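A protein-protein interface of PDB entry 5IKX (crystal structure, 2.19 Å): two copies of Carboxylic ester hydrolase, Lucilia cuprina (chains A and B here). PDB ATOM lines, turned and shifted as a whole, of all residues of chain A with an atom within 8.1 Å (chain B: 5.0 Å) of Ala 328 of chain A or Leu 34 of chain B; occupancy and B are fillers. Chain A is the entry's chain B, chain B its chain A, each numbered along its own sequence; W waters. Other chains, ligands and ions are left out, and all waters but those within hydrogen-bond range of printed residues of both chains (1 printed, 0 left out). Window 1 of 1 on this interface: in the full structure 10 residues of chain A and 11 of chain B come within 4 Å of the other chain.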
ATOM      1  N   ALA A  82      17.811 -19.601   1.107  1.00  0.00           N
ATOM      2  CA  ALA A  82      17.753 -21.054   1.039  1.00  0.00           C
ATOM      3  C   ALA A  82      19.168 -21.613   1.088  1.00  0.00           C
ATOM      4  O   ALA A  82      20.101 -20.962   0.600  1.00  0.00           O
ATOM      5  CB  ALA A  82      17.061 -21.480  -0.242  1.00  0.00           C
ATOM      6  N   ASN A 188      14.286 -12.560  -2.696  1.00  0.00           N
ATOM      7  CA  ASN A 188      14.616 -13.978  -2.498  1.00  0.00           C
ATOM      8  C   ASN A 188      14.746 -14.323  -1.004  1.00  0.00           C
ATOM      9  O   ASN A 188      15.610 -15.099  -0.609  1.00  0.00           O
ATOM     10  CB  ASN A 188      15.891 -14.356  -3.276  1.00  0.00           C
ATOM     11  CG  ASN A 188      15.920 -15.817  -3.715  1.00  0.00           C
ATOM     12  OD1 ASN A 188      14.926 -16.362  -4.221  1.00  0.00           O
ATOM     13  ND2 ASN A 188      17.082 -16.454  -3.553  1.00  0.00           N
ATOM     14  N   PRO A 190      11.786 -15.534   0.902  1.00  0.00           N
ATOM     15  CA  PRO A 190      10.390 -15.918   1.147  1.00  0.00           C
ATOM     16  C   PRO A 190      10.085 -16.384   2.582  1.00  0.00           C
ATOM     17  O   PRO A 190       8.937 -16.288   3.024  1.00  0.00           O
ATOM     18  CB  PRO A 190      10.161 -17.071   0.165  1.00  0.00           C
ATOM     19  CG  PRO A 190      11.509 -17.591  -0.162  1.00  0.00           C
ATOM     20  CD  PRO A 190      12.417 -16.399  -0.112  1.00  0.00           C
ATOM     21  N   LYS A 196      14.034 -25.402   4.892  1.00  0.00           N
ATOM     22  CA  LYS A 196      14.702 -25.803   3.660  1.00  0.00           C
ATOM     23  C   LYS A 196      16.080 -26.395   3.964  1.00  0.00           C
ATOM     24  O   LYS A 196      16.605 -27.168   3.172  1.00  0.00           O
ATOM     25  CB  LYS A 196      14.835 -24.615   2.698  1.00  0.00           C
ATOM     26  CG  LYS A 196      13.511 -24.026   2.228  1.00  0.00           C
ATOM     27  CD  LYS A 196      13.717 -22.631   1.643  1.00  0.00           C
ATOM     28  CE  LYS A 196      12.500 -22.130   0.876  1.00  0.00           C
ATOM     29  NZ  LYS A 196      11.271 -22.105   1.722  1.00  0.00           N
ATOM     30  N   ARG A 203      17.687 -34.787   2.275  1.00  0.00           N
ATOM     31  CA  ARG A 203      18.157 -35.188   0.947  1.00  0.00           C
ATOM     32  C   ARG A 203      19.544 -35.819   1.001  1.00  0.00           C
ATOM     33  O   ARG A 203      19.797 -36.827   0.350  1.00  0.00           O
ATOM     34  CB  ARG A 203      18.152 -34.010  -0.032  1.00  0.00           C
ATOM     35  CG  ARG A 203      16.807 -33.778  -0.681  1.00  0.00           C
ATOM     36  CD  ARG A 203      16.847 -32.617  -1.654  1.00  0.00           C
ATOM     37  NE  ARG A 203      15.505 -32.352  -2.170  1.00  0.00           N
ATOM     38  CZ  ARG A 203      15.030 -31.149  -2.482  1.00  0.00           C
ATOM     39  NH1 ARG A 203      15.788 -30.074  -2.341  1.00  0.00           N
ATOM     40  NH2 ARG A 203      13.787 -31.031  -2.932  1.00  0.00           N
ATOM     41  N   GLN A 239       8.543 -30.919  -1.623  1.00  0.00           N
ATOM     42  CA  GLN A 239      10.000 -31.021  -1.695  1.00  0.00           C
ATOM     43  C   GLN A 239      10.534 -32.394  -1.257  1.00  0.00           C
ATOM     44  O   GLN A 239      11.459 -32.920  -1.858  1.00  0.00           O
ATOM     45  CB  GLN A 239      10.670 -29.929  -0.850  1.00  0.00           C
ATOM     46  CG  GLN A 239      10.413 -28.492  -1.293  1.00  0.00           C
ATOM     47  CD  GLN A 239      10.876 -28.190  -2.707  1.00  0.00           C
ATOM     48  OE1 GLN A 239      11.710 -28.894  -3.282  1.00  0.00           O
ATOM     49  NE2 GLN A 239      10.339 -27.124  -3.273  1.00  0.00           N
ATOM     50  N   GLU A 323       4.594 -18.956   2.465  1.00  0.00           N
ATOM     51  CA  GLU A 323       5.497 -18.134   1.669  1.00  0.00           C
ATOM     52  C   GLU A 323       4.720 -17.262   0.665  1.00  0.00           C
ATOM     53  O   GLU A 323       3.864 -17.767  -0.055  1.00  0.00           O
ATOM     54  CB  GLU A 323       6.578 -19.001   1.005  1.00  0.00           C
ATOM     55  CG  GLU A 323       7.436 -19.736   2.035  1.00  0.00           C
ATOM     56  CD  GLU A 323       8.467 -20.678   1.441  1.00  0.00           C
ATOM     57  OE1 GLU A 323       8.445 -21.886   1.797  1.00  0.00           O
ATOM     58  OE2 GLU A 323       9.310 -20.223   0.632  1.00  0.00           O
ATOM     59  N   TYR A 325       5.178 -15.820  -2.168  1.00  0.00           N
ATOM     60  CA  TYR A 325       5.283 -16.030  -3.609  1.00  0.00           C
ATOM     61  C   TYR A 325       6.020 -17.344  -3.824  1.00  0.00           C
ATOM     62  O   TYR A 325       6.746 -17.807  -2.935  1.00  0.00           O
ATOM     63  CB  TYR A 325       6.042 -14.871  -4.278  1.00  0.00           C
ATOM     64  CG  TYR A 325       7.406 -14.608  -3.661  1.00  0.00           C
ATOM     65  CD1 TYR A 325       8.556 -15.249  -4.142  1.00  0.00           C
ATOM     66  CD2 TYR A 325       7.543 -13.727  -2.593  1.00  0.00           C
ATOM     67  CE1 TYR A 325       9.796 -15.004  -3.572  1.00  0.00           C
ATOM     68  CE2 TYR A 325       8.774 -13.483  -2.015  1.00  0.00           C
ATOM     69  CZ  TYR A 325       9.896 -14.119  -2.500  1.00  0.00           C
ATOM     70  OH  TYR A 325      11.117 -13.868  -1.907  1.00  0.00           O
ATOM     71  N   GLN A 326       5.844 -17.939  -4.997  1.00  0.00           N
ATOM     72  CA  GLN A 326       6.495 -19.202  -5.313  1.00  0.00           C
ATOM     73  C   GLN A 326       7.971 -19.040  -5.693  1.00  0.00           C
ATOM     74  O   GLN A 326       8.352 -18.071  -6.358  1.00  0.00           O
ATOM     75  CB  GLN A 326       5.738 -19.955  -6.417  1.00  0.00           C
ATOM     76  CG  GLN A 326       6.256 -21.370  -6.629  1.00  0.00           C
ATOM     77  CD  GLN A 326       5.483 -22.164  -7.656  1.00  0.00           C
ATOM     78  OE1 GLN A 326       4.341 -21.848  -7.983  1.00  0.00           O
ATOM     79  NE2 GLN A 326       6.105 -23.224  -8.163  1.00  0.00           N
ATOM     80  N   THR A 327       8.788 -19.986  -5.225  1.00  0.00           N
ATOM     81  CA  THR A 327      10.178 -20.148  -5.654  1.00  0.00           C
ATOM     82  C   THR A 327      10.426 -21.637  -5.898  1.00  0.00           C
ATOM     83  O   THR A 327       9.559 -22.472  -5.590  1.00  0.00           O
ATOM     84  CB  THR A 327      11.193 -19.635  -4.616  1.00  0.00           C
ATOM     85  OG1 THR A 327      10.997 -20.314  -3.366  1.00  0.00           O
ATOM     86  CG2 THR A 327      11.082 -18.120  -4.422  1.00  0.00           C
ATOM     87  N   ALA A 328      11.594 -21.958  -6.457  1.00  0.00           N
ATOM     88  CA  ALA A 328      12.001 -23.351  -6.712  1.00  0.00           C
ATOM     89  C   ALA A 328      12.071 -24.201  -5.438  1.00  0.00           C
ATOM     90  O   ALA A 328      11.697 -25.373  -5.449  1.00  0.00           O
ATOM     91  CB  ALA A 328      13.342 -23.390  -7.428  1.00  0.00           C
ATOM     92  N   ASP A 329      12.535 -23.584  -4.360  1.00  0.00           N
ATOM     93  CA  ASP A 329      12.809 -24.256  -3.094  1.00  0.00           C
ATOM     94  C   ASP A 329      11.703 -24.084  -2.048  1.00  0.00           C
ATOM     95  O   ASP A 329      11.920 -24.386  -0.871  1.00  0.00           O
ATOM     96  CB  ASP A 329      14.136 -23.754  -2.526  1.00  0.00           C
ATOM     97  CG  ASP A 329      15.329 -24.159  -3.375  1.00  0.00           C
ATOM     98  OD1 ASP A 329      15.226 -25.138  -4.139  1.00  0.00           O
ATOM     99  OD2 ASP A 329      16.377 -23.483  -3.284  1.00  0.00           O
ATOM    100  N   CYS A 330      10.535 -23.611  -2.492  1.00  0.00           N
ATOM    101  CA  CYS A 330       9.363 -23.356  -1.652  1.00  0.00           C
ATOM    102  C   CYS A 330       8.888 -24.601  -0.912  1.00  0.00           C
ATOM    103  O   CYS A 330       8.503 -25.605  -1.525  1.00  0.00           O
ATOM    104  CB  CYS A 330       8.214 -22.795  -2.509  1.00  0.00           C
ATOM    105  SG  CYS A 330       6.712 -22.371  -1.585  1.00  0.00           S
ATOM    106  N   VAL A 331       8.901 -24.519   0.410  1.00  0.00           N
ATOM    107  CA  VAL A 331       8.465 -25.619   1.270  1.00  0.00           C
ATOM    108  C   VAL A 331       6.987 -25.497   1.698  1.00  0.00           C
ATOM    109  O   VAL A 331       6.276 -26.502   1.739  1.00  0.00           O
ATOM    110  CB  VAL A 331       9.414 -25.768   2.492  1.00  0.00           C
ATOM    111  CG1 VAL A 331       8.806 -26.665   3.572  1.00  0.00           C
ATOM    112  CG2 VAL A 331      10.755 -26.327   2.033  1.00  0.00           C
ATOM    113  N   LEU B  30      10.276 -32.644 -10.092  1.00  0.00           N
ATOM    114  CA  LEU B  30      10.935 -31.336 -10.149  1.00  0.00           C
ATOM    115  C   LEU B  30      10.173 -30.419 -11.118  1.00  0.00           C
ATOM    116  O   LEU B  30       9.975 -29.244 -10.829  1.00  0.00           O
ATOM    117  CB  LEU B  30      12.415 -31.470 -10.556  1.00  0.00           C
ATOM    118  CG  LEU B  30      13.258 -30.211 -10.843  1.00  0.00           C
ATOM    119  CD1 LEU B  30      13.410 -29.290  -9.642  1.00  0.00           C
ATOM    120  CD2 LEU B  30      14.632 -30.604 -11.371  1.00  0.00           C
ATOM    121  N   ASN B  31       9.731 -30.984 -12.243  1.00  0.00           N
ATOM    122  CA  ASN B  31       8.900 -30.276 -13.228  1.00  0.00           C
ATOM    123  C   ASN B  31       7.619 -29.717 -12.601  1.00  0.00           C
ATOM    124  O   ASN B  31       7.251 -28.578 -12.894  1.00  0.00           O
ATOM    125  CB  ASN B  31       8.568 -31.187 -14.415  1.00  0.00           C
ATOM    126  CG  ASN B  31       8.016 -30.425 -15.612  1.00  0.00           C
ATOM    127  OD1 ASN B  31       8.749 -29.739 -16.322  1.00  0.00           O
ATOM    128  ND2 ASN B  31       6.716 -30.562 -15.851  1.00  0.00           N
ATOM    129  N   TYR B  32       6.971 -30.507 -11.727  1.00  0.00           N
ATOM    130  CA  TYR B  32       5.772 -30.070 -11.005  1.00  0.00           C
ATOM    131  C   TYR B  32       6.095 -28.977 -10.003  1.00  0.00           C
ATOM    132  O   TYR B  32       5.372 -27.994  -9.927  1.00  0.00           O
ATOM    133  CB  TYR B  32       5.074 -31.218 -10.264  1.00  0.00           C
ATOM    134  CG  TYR B  32       4.538 -32.324 -11.137  1.00  0.00           C
ATOM    135  CD1 TYR B  32       4.594 -33.653 -10.712  1.00  0.00           C
ATOM    136  CD2 TYR B  32       3.979 -32.051 -12.384  1.00  0.00           C
ATOM    137  CE1 TYR B  32       4.104 -34.678 -11.505  1.00  0.00           C
ATOM    138  CE2 TYR B  32       3.494 -33.066 -13.187  1.00  0.00           C
ATOM    139  CZ  TYR B  32       3.556 -34.378 -12.743  1.00  0.00           C
ATOM    140  OH  TYR B  32       3.062 -35.386 -13.545  1.00  0.00           O
ATOM    141  N   ARG B  33       7.173 -29.161  -9.237  1.00  0.00           N
ATOM    142  CA  ARG B  33       7.656 -28.138  -8.316  1.00  0.00           C
ATOM    143  C   ARG B  33       7.965 -26.817  -9.043  1.00  0.00           C
ATOM    144  O   ARG B  33       7.693 -25.738  -8.526  1.00  0.00           O
ATOM    145  CB  ARG B  33       8.868 -28.639  -7.514  1.00  0.00           C
ATOM    146  CG  ARG B  33       8.547 -29.750  -6.519  1.00  0.00           C
ATOM    147  CD  ARG B  33       9.715 -30.079  -5.599  1.00  0.00           C
ATOM    148  NE  ARG B  33      10.692 -30.999  -6.195  1.00  0.00           N
ATOM    149  CZ  ARG B  33      11.992 -30.744  -6.307  1.00  0.00           C
ATOM    150  NH1 ARG B  33      12.499 -29.595  -5.871  1.00  0.00           N
ATOM    151  NH2 ARG B  33      12.797 -31.638  -6.852  1.00  0.00           N
ATOM    152  N   LEU B  34       8.505 -26.902 -10.253  1.00  0.00           N
ATOM    153  CA  LEU B  34       8.801 -25.696 -11.035  1.00  0.00           C
ATOM    154  C   LEU B  34       7.617 -25.118 -11.827  1.00  0.00           C
ATOM    155  O   LEU B  34       7.814 -24.294 -12.716  1.00  0.00           O
ATOM    156  CB  LEU B  34       9.981 -25.949 -11.972  1.00  0.00           C
ATOM    157  CG  LEU B  34      11.341 -26.225 -11.325  1.00  0.00           C
ATOM    158  CD1 LEU B  34      12.351 -26.631 -12.389  1.00  0.00           C
ATOM    159  CD2 LEU B  34      11.817 -25.016 -10.536  1.00  0.00           C
ATOM    160  N   THR B  35       6.395 -25.531 -11.506  1.00  0.00           N
ATOM    161  CA  THR B  35       5.216 -25.089 -12.267  1.00  0.00           C
ATOM    162  C   THR B  35       4.329 -24.140 -11.473  1.00  0.00           C
ATOM    163  O   THR B  35       3.898 -24.453 -10.365  1.00  0.00           O
ATOM    164  CB  THR B  35       4.398 -26.282 -12.804  1.00  0.00           C
ATOM    165  OG1 THR B  35       5.223 -27.061 -13.672  1.00  0.00           O
ATOM    166  CG2 THR B  35       3.178 -25.811 -13.603  1.00  0.00           C
ATOM    167  N   THR B  36       4.083 -22.972 -12.055  1.00  0.00           N
ATOM    168  CA  THR B  36       3.229 -21.944 -11.463  1.00  0.00           C
ATOM    169  C   THR B  36       1.761 -22.235 -11.764  1.00  0.00           C
ATOM    170  O   THR B  36       1.447 -23.127 -12.561  1.00  0.00           O
ATOM    171  CB  THR B  36       3.622 -20.551 -12.013  1.00  0.00           C
ATOM    172  OG1 THR B  36       5.052 -20.418 -11.991  1.00  0.00           O
ATOM    173  CG2 THR B  36       3.039 -19.438 -11.187  1.00  0.00           C
ATOM    174  N   LYS B  53       3.365 -20.343 -17.104  1.00  0.00           N
ATOM    175  CA  LYS B  53       4.540 -19.746 -16.499  1.00  0.00           C
ATOM    176  C   LYS B  53       5.209 -20.802 -15.615  1.00  0.00           C
ATOM    177  O   LYS B  53       4.566 -21.407 -14.748  1.00  0.00           O
ATOM    178  CB  LYS B  53       4.153 -18.524 -15.675  1.00  0.00           C
ATOM    179  CG  LYS B  53       5.313 -17.628 -15.274  1.00  0.00           C
ATOM    180  CD  LYS B  53       4.977 -16.891 -13.985  1.00  0.00           C
ATOM    181  CE  LYS B  53       5.854 -15.670 -13.762  1.00  0.00           C
ATOM    182  NZ  LYS B  53       5.684 -15.146 -12.374  1.00  0.00           N
ATOM    183  N   ARG B  54       6.499 -21.018 -15.863  1.00  0.00           N
ATOM    184  CA  ARG B  54       7.288 -22.031 -15.178  1.00  0.00           C
ATOM    185  C   ARG B  54       8.506 -21.395 -14.573  1.00  0.00           C
ATOM    186  O   ARG B  54       9.126 -20.535 -15.188  1.00  0.00           O
ATOM    187  CB  ARG B  54       7.800 -23.070 -16.164  1.00  0.00           C
ATOM    188  CG  ARG B  54       6.738 -23.731 -16.999  1.00  0.00           C
ATOM    189  CD  ARG B  54       7.406 -24.705 -17.940  1.00  0.00           C
ATOM    190  NE  ARG B  54       6.410 -25.399 -18.733  1.00  0.00           N
ATOM    191  CZ  ARG B  54       5.740 -26.468 -18.335  1.00  0.00           C
ATOM    192  NH1 ARG B  54       5.967 -27.000 -17.142  1.00  0.00           N
ATOM    193  NH2 ARG B  54       4.852 -27.013 -19.152  1.00  0.00           N
ATOM    194  N   LEU B  55       8.872 -21.866 -13.383  1.00  0.00           N
ATOM    195  CA  LEU B  55      10.078 -21.410 -12.715  1.00  0.00           C
ATOM    196  C   LEU B  55      11.323 -22.188 -13.148  1.00  0.00           C
ATOM    197  O   LEU B  55      11.235 -23.199 -13.849  1.00  0.00           O
ATOM    198  CB  LEU B  55       9.905 -21.466 -11.199  1.00  0.00           C
ATOM    199  CG  LEU B  55       8.900 -20.488 -10.588  1.00  0.00           C
ATOM    200  CD1 LEU B  55       8.828 -20.694  -9.085  1.00  0.00           C
ATOM    201  CD2 LEU B  55       9.257 -19.044 -10.917  1.00  0.00           C
ATOM    202  N   THR B  56      12.468 -21.691 -12.689  1.00  0.00           N
ATOM    203  CA  THR B  56      13.804 -22.150 -13.055  1.00  0.00           C
ATOM    204  C   THR B  56      14.536 -22.412 -11.730  1.00  0.00           C
ATOM    205  O   THR B  56      14.173 -21.811 -10.721  1.00  0.00           O
ATOM    206  CB  THR B  56      14.476 -21.017 -13.863  1.00  0.00           C
ATOM    207  OG1 THR B  56      14.422 -21.300 -15.274  1.00  0.00           O
ATOM    208  CG2 THR B  56      15.869 -20.762 -13.434  1.00  0.00           C
ATOM    209  N   VAL B  57      15.560 -23.274 -11.697  1.00  0.00           N
ATOM    210  CA  VAL B  57      16.291 -23.480 -10.409  1.00  0.00           C
ATOM    211  C   VAL B  57      16.923 -22.205  -9.849  1.00  0.00           C
ATOM    212  O   VAL B  57      17.137 -22.080  -8.631  1.00  0.00           O
ATOM    213  CB  VAL B  57      17.340 -24.624 -10.430  1.00  0.00           C
ATOM    214  CG1 VAL B  57      16.659 -25.970 -10.636  1.00  0.00           C
ATOM    215  CG2 VAL B  57      18.442 -24.368 -11.455  1.00  0.00           C
ATOM    216  N   ASP B  59      15.455 -19.427 -10.038  1.00  0.00           N
ATOM    217  CA  ASP B  59      14.278 -18.602  -9.752  1.00  0.00           C
ATOM    218  C   ASP B  59      14.027 -17.478 -10.758  1.00  0.00           C
ATOM    219  O   ASP B  59      13.639 -16.360 -10.395  1.00  0.00           O
ATOM    220  CB  ASP B  59      14.289 -18.078  -8.305  1.00  0.00           C
ATOM    221  CG  ASP B  59      13.680 -19.063  -7.327  1.00  0.00           C
ATOM    222  OD1 ASP B  59      13.009 -20.023  -7.769  1.00  0.00           O
ATOM    223  OD2 ASP B  59      13.877 -18.876  -6.109  1.00  0.00           O
HETATM  224  O   HOH W   1       8.062 -24.694  -6.076  1.00  0.00           O
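NH1 of Arg 33 of chain B is in hydrogen-bond range of OE1 of Gln 239 of chain A (2.8 Å).
The side-chain amide nitrogen (NE2) of Gln 326 of chain A sits at hydrogen-bond distance from the backbone carbonyl oxygen (O) of Arg 33 of chain B (3.0 Å).
The backbone carbonyl oxygen (O) of Thr 35 of chain B sits at hydrogen-bond distance from the side-chain amide nitrogen (NE2) of Gln 326 of chain A.
The side-chain amide oxygen of Asn 188 of chain A lies close to the side-chain carboxylate of Asp 59 of chain B.
The backbone NH (N) of Ala 328 of chain A is in hydrogen-bond range of the side-chain carboxylate (OD1) of Asp 59 of chain B, at 2.7 Å.
The backbone carbonyl oxygen (O) of Asn 31 of chain B lies within hydrogen-bond range of the side-chain hydroxyl (OG1) of Thr 35 of chain B (2.6 Å).
The backbone carbonyl oxygen (O) of Leu 34 of chain B sits at hydrogen-bond distance from the backbone NH (N) of Leu 55 of chain B (2.7 Å).
The backbone carbonyl oxygen of Lys 53 of chain B lies within hydrogen-bond range of the side-chain hydroxyl of Thr 36 of chain B (3.0 Å).
The guanidinium group (NH2) of Arg 203 of chain A is in hydrogen-bond range of the side-chain amide oxygen (OE1) of Gln 239 of chain A (3.0 Å).
O of Ala 328 of chain A is in hydrogen-bond range of NE2 of Gln 239 of chain A, at 3.1 Å.
OG1 of Thr 327 of chain A lies within hydrogen-bond range of N of Cys 330 of chain A (3.4 Å).
Among the printed residues, pairs that only touch across the chains: Thr 327 of chain A with Asp 59 of chain B, Arg 203 of chain A with Arg 33 of chain B, Gln 326 of chain A with Leu 55 of chain B, Gln 326 of chain A with Thr 36 of chain B, Thr 327 of chain A with Leu 55 of chain B, Ala 328 of chain A with Thr 56 of chain B and Ala 328 of chain A with Leu 34 of chain B.
Of the printed residues of chain B, Gln 239 of chain A touches Arg 33 (2.8 Å).
Of the printed residues of chain A, Arg 33 of chain B touches Arg 203, Gln 239 and Gln 326.
Leu 34 of chain B touches just one residue of chain A: Ala 328 (3.8 Å).
The nearest printed residue of chain B that does not touch Ala 328 of chain A is Leu 55 of chain B (4.02 Å).
Of the 14 printed residues of chain A, 6 touch a printed residue of chain B.
Printed residues of chain A that touch a printed residue of chain B: Asn 188, Arg 203, Gln 239, Gln 326, Thr 327 and Ala 328.
Hydrophobic or aromatic side chains of chain A within 4 Å of the printed part of chain B: Ala 328.
Of the 13 printed residues of chain B, 7 touch a printed residue of chain A.
Printed residues of chain B that touch a printed residue of chain A: Arg 33, Leu 34, Thr 35, Thr 36, Leu 55, Thr 56 and Asp 59.
Among the printed residues, 12 pairs touch across the chains.
Among the printed residues, no Asp or Glu carboxylate lies within 4 Å of a Lys or Arg side-chain nitrogen of the other chain.
No position is printed for both chains.
Water W1 lies within hydrogen-bond range of O of Arg 33 of chain B (2.7 Å), O of Thr 327 of chain A (2.7 Å) and NE2 of Gln 326 of chain A (3.2 Å).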
